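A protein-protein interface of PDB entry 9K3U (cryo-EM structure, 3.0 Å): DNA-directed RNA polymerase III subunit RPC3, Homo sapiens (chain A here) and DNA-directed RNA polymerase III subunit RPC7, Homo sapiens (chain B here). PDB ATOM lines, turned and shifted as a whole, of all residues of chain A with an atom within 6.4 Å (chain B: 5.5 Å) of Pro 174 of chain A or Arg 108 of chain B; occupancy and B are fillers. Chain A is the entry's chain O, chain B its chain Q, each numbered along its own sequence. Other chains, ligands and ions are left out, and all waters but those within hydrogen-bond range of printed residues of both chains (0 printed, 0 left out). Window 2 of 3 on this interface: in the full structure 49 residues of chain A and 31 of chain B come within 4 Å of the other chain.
O of Pro 175 of chain A sits at hydrogen-bond distance from NH2 of Arg 108 of chain B (3.1 Å).
The side-chain amino group of Lys 51 of chain A lies within hydrogen-bond range of the backbone carbonyl oxygen of Met 111 of chain B (3.4 Å).
NH2 of Arg 113 of chain B lies close to NZ of Lys 51 of chain A (2.9 Å).
The guanidinium group (NH2) of Arg 108 of chain B lies within hydrogen-bond range of the backbone carbonyl oxygen (O) of Pro 174 of chain A (2.5 Å).
The backbone carbonyl oxygen of Arg 108 of chain B lies within hydrogen-bond range of the guanidinium group of Arg 113 of chain B (3.1 Å).
O of Met 111 of chain B lies within hydrogen-bond range of NH1 of Arg 113 of chain B.
Lys 51 of chain A touches Glu 109 of chain B (CE to O, 3.1 Å).
Met 110 of chain B touches Lys 51 of chain A.
Pro 107 of chain B touches Pro 176 of chain A.
NH1 of Arg 108 of chain B touches CA of Pro 176 of chain A, 3.4 Å away.
Of chain B, only Arg 108 comes within 4 Å of Pro 174 of chain A.
Arg 108 of chain B touches just these residues of chain A: Pro 174 (2.5 Å), Pro 175 (3.1 Å) and Pro 176 (3.4 Å).
Printed residues of chain B within 4 Å of Lys 51 of chain A: Glu 109, Met 110, Met 111 and Arg 113.
Of the printed residues of chain A, Met 110 of chain B touches Lys 51.
Gly 172 of chain A touches none of the printed residues of chain B.
Pro 173 of chain A touches none of the printed residues of chain B.
The nearest printed residue of chain A that does not touch Glu 109 of chain B is Pro 176 of chain A (4.9 Å).
Along chain A the printed residues that touch a printed residue of chain B span positions 51 to 176.
Of the 7 printed residues of chain B, 6 touch a printed residue of chain A.
Among the printed residues, 8 pairs touch across the chains.
Among the printed residues, no Asp or Glu carboxylate lies within 4 Å of a Lys or Arg side-chain nitrogen of the other chain.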
ATOM      1  N   LYS A  51     -22.843 -16.772   9.315  1.00  0.00           N
ATOM      2  CA  LYS A  51     -23.825 -15.830   9.844  1.00  0.00           C
ATOM      3  C   LYS A  51     -25.066 -16.555  10.347  1.00  0.00           C
ATOM      4  O   LYS A  51     -25.578 -16.246  11.427  1.00  0.00           O
ATOM      5  CB  LYS A  51     -24.207 -14.810   8.770  1.00  0.00           C
ATOM      6  CG  LYS A  51     -23.091 -13.854   8.382  1.00  0.00           C
ATOM      7  CD  LYS A  51     -23.521 -12.958   7.232  1.00  0.00           C
ATOM      8  CE  LYS A  51     -22.378 -12.084   6.741  1.00  0.00           C
ATOM      9  NZ  LYS A  51     -22.799 -11.195   5.625  1.00  0.00           N
ATOM     10  N   GLY A 172     -27.364   9.208  16.474  1.00  0.00           N
ATOM     11  CA  GLY A 172     -26.445   9.487  15.397  1.00  0.00           C
ATOM     12  C   GLY A 172     -26.060   8.232  14.638  1.00  0.00           C
ATOM     13  O   GLY A 172     -26.904   7.373  14.358  1.00  0.00           O
ATOM     14  N   PRO A 173     -24.785   8.096  14.285  1.00  0.00           N
ATOM     15  CA  PRO A 173     -24.340   6.901  13.559  1.00  0.00           C
ATOM     16  C   PRO A 173     -24.648   5.638  14.345  1.00  0.00           C
ATOM     17  O   PRO A 173     -24.345   5.559  15.546  1.00  0.00           O
ATOM     18  CB  PRO A 173     -22.827   7.113  13.417  1.00  0.00           C
ATOM     19  CG  PRO A 173     -22.642   8.582  13.494  1.00  0.00           C
ATOM     20  CD  PRO A 173     -23.694   9.076  14.441  1.00  0.00           C
ATOM     21  N   PRO A 174     -25.243   4.629  13.715  1.00  0.00           N
ATOM     22  CA  PRO A 174     -25.559   3.392  14.434  1.00  0.00           C
ATOM     23  C   PRO A 174     -24.306   2.575  14.690  1.00  0.00           C
ATOM     24  O   PRO A 174     -23.484   2.392  13.778  1.00  0.00           O
ATOM     25  CB  PRO A 174     -26.518   2.665  13.483  1.00  0.00           C
ATOM     26  CG  PRO A 174     -26.130   3.148  12.132  1.00  0.00           C
ATOM     27  CD  PRO A 174     -25.687   4.573  12.310  1.00  0.00           C
ATOM     28  N   PRO A 175     -24.115   2.070  15.905  1.00  0.00           N
ATOM     29  CA  PRO A 175     -22.908   1.291  16.201  1.00  0.00           C
ATOM     30  C   PRO A 175     -22.990  -0.095  15.584  1.00  0.00           C
ATOM     31  O   PRO A 175     -24.082  -0.560  15.230  1.00  0.00           O
ATOM     32  CB  PRO A 175     -22.900   1.225  17.732  1.00  0.00           C
ATOM     33  CG  PRO A 175     -24.334   1.297  18.108  1.00  0.00           C
ATOM     34  CD  PRO A 175     -24.989   2.192  17.086  1.00  0.00           C
ATOM     35  N   PRO A 176     -21.853  -0.782  15.437  1.00  0.00           N
ATOM     36  CA  PRO A 176     -21.903  -2.145  14.885  1.00  0.00           C
ATOM     37  C   PRO A 176     -22.796  -3.084  15.672  1.00  0.00           C
ATOM     38  O   PRO A 176     -23.448  -3.950  15.073  1.00  0.00           O
ATOM     39  CB  PRO A 176     -20.434  -2.593  14.930  1.00  0.00           C
ATOM     40  CG  PRO A 176     -19.651  -1.326  14.926  1.00  0.00           C
ATOM     41  CD  PRO A 176     -20.473  -0.338  15.689  1.00  0.00           C
ATOM     42  N   ALA A 177     -22.850  -2.940  16.996  1.00  0.00           N
ATOM     43  CA  ALA A 177     -23.692  -3.769  17.836  1.00  0.00           C
ATOM     44  C   ALA A 177     -24.597  -2.900  18.700  1.00  0.00           C
ATOM     45  O   ALA A 177     -24.167  -1.844  19.177  1.00  0.00           O
ATOM     46  CB  ALA A 177     -22.846  -4.680  18.742  1.00  0.00           C
ATOM     47  N   PRO A 178     -25.854  -3.304  18.917  1.00  0.00           N
ATOM     48  CA  PRO A 178     -26.752  -2.492  19.753  1.00  0.00           C
ATOM     49  C   PRO A 178     -26.368  -2.460  21.223  1.00  0.00           C
ATOM     50  O   PRO A 178     -26.878  -1.605  21.956  1.00  0.00           O
ATOM     51  CB  PRO A 178     -28.119  -3.161  19.553  1.00  0.00           C
ATOM     52  CG  PRO A 178     -27.801  -4.563  19.167  1.00  0.00           C
ATOM     53  CD  PRO A 178     -26.528  -4.501  18.382  1.00  0.00           C
ATOM     54  N   LEU B 106     -29.738  -8.172  16.736  1.00  0.00           N
ATOM     55  CA  LEU B 106     -28.563  -8.773  16.117  1.00  0.00           C
ATOM     56  C   LEU B 106     -27.749  -7.704  15.386  1.00  0.00           C
ATOM     57  O   LEU B 106     -28.322  -6.846  14.711  1.00  0.00           O
ATOM     58  CB  LEU B 106     -28.980  -9.868  15.138  1.00  0.00           C
ATOM     59  CG  LEU B 106     -27.867 -10.777  14.606  1.00  0.00           C
ATOM     60  CD1 LEU B 106     -27.316 -11.667  15.712  1.00  0.00           C
ATOM     61  CD2 LEU B 106     -28.377 -11.614  13.445  1.00  0.00           C
ATOM     62  N   PRO B 107     -26.421  -7.720  15.504  1.00  0.00           N
ATOM     63  CA  PRO B 107     -25.606  -6.733  14.786  1.00  0.00           C
ATOM     64  C   PRO B 107     -25.846  -6.794  13.285  1.00  0.00           C
ATOM     65  O   PRO B 107     -26.493  -7.703  12.758  1.00  0.00           O
ATOM     66  CB  PRO B 107     -24.166  -7.120  15.143  1.00  0.00           C
ATOM     67  CG  PRO B 107     -24.280  -7.866  16.422  1.00  0.00           C
ATOM     68  CD  PRO B 107     -25.594  -8.585  16.367  1.00  0.00           C
ATOM     69  N   ARG B 108     -25.303  -5.795  12.585  1.00  0.00           N
ATOM     70  CA  ARG B 108     -25.506  -5.696  11.145  1.00  0.00           C
ATOM     71  C   ARG B 108     -24.655  -6.679  10.354  1.00  0.00           C
ATOM     72  O   ARG B 108     -24.898  -6.856   9.154  1.00  0.00           O
ATOM     73  CB  ARG B 108     -25.210  -4.269  10.667  1.00  0.00           C
ATOM     74  CG  ARG B 108     -23.740  -3.859  10.742  1.00  0.00           C
ATOM     75  CD  ARG B 108     -23.506  -2.532  10.038  1.00  0.00           C
ATOM     76  NE  ARG B 108     -24.007  -1.397  10.812  1.00  0.00           N
ATOM     77  CZ  ARG B 108     -23.264  -0.637  11.616  1.00  0.00           C
ATOM     78  NH1 ARG B 108     -21.968  -0.873  11.764  1.00  0.00           N
ATOM     79  NH2 ARG B 108     -23.825   0.370  12.272  1.00  0.00           N
ATOM     80  N   GLU B 109     -23.672  -7.321  10.984  1.00  0.00           N
ATOM     81  CA  GLU B 109     -22.765  -8.214  10.277  1.00  0.00           C
ATOM     82  C   GLU B 109     -23.388  -9.561   9.931  1.00  0.00           C
ATOM     83  O   GLU B 109     -22.695 -10.413   9.365  1.00  0.00           O
ATOM     84  CB  GLU B 109     -21.501  -8.440  11.110  1.00  0.00           C
ATOM     85  CG  GLU B 109     -20.719  -7.170  11.406  1.00  0.00           C
ATOM     86  CD  GLU B 109     -19.469  -7.429  12.222  1.00  0.00           C
ATOM     87  OE1 GLU B 109     -19.216  -8.604  12.570  1.00  0.00           O
ATOM     88  OE2 GLU B 109     -18.736  -6.461  12.515  1.00  0.00           O
ATOM     89  N   MET B 110     -24.664  -9.777  10.253  1.00  0.00           N
ATOM     90  CA  MET B 110     -25.329 -11.050   9.996  1.00  0.00           C
ATOM     91  C   MET B 110     -26.477 -10.929   9.000  1.00  0.00           C
ATOM     92  O   MET B 110     -27.214 -11.899   8.804  1.00  0.00           O
ATOM     93  CB  MET B 110     -25.839 -11.651  11.307  1.00  0.00           C
ATOM     94  CG  MET B 110     -24.801 -12.470  12.060  1.00  0.00           C
ATOM     95  SD  MET B 110     -23.364 -11.512  12.580  1.00  0.00           S
ATOM     96  CE  MET B 110     -24.113 -10.394  13.759  1.00  0.00           C
ATOM     97  N   MET B 111     -26.651  -9.768   8.363  1.00  0.00           N
ATOM     98  CA  MET B 111     -27.696  -9.662   7.354  1.00  0.00           C
ATOM     99  C   MET B 111     -27.244 -10.336   6.057  1.00  0.00           C
ATOM    100  O   MET B 111     -26.071 -10.242   5.687  1.00  0.00           O
ATOM    101  CB  MET B 111     -28.046  -8.199   7.076  1.00  0.00           C
ATOM    102  CG  MET B 111     -29.168  -7.645   7.947  1.00  0.00           C
ATOM    103  SD  MET B 111     -28.578  -6.802   9.425  1.00  0.00           S
ATOM    104  CE  MET B 111     -27.855  -5.332   8.702  1.00  0.00           C
ATOM    105  N   ARG B 113     -28.195  -9.529   2.933  1.00  0.00           N
ATOM    106  CA  ARG B 113     -28.065  -8.550   1.856  1.00  0.00           C
ATOM    107  C   ARG B 113     -28.153  -9.231   0.493  1.00  0.00           C
ATOM    108  O   ARG B 113     -28.752  -8.702  -0.440  1.00  0.00           O
ATOM    109  CB  ARG B 113     -26.750  -7.776   1.969  1.00  0.00           C
ATOM    110  CG  ARG B 113     -26.719  -6.751   3.096  1.00  0.00           C
ATOM    111  CD  ARG B 113     -26.137  -7.329   4.370  1.00  0.00           C
ATOM    112  NE  ARG B 113     -24.717  -7.638   4.232  1.00  0.00           N
ATOM    113  CZ  ARG B 113     -23.946  -8.093   5.216  1.00  0.00           C
ATOM    114  NH1 ARG B 113     -24.454  -8.298   6.424  1.00  0.00           N
ATOM    115  NH2 ARG B 113     -22.664  -8.344   4.990  1.00  0.00           N
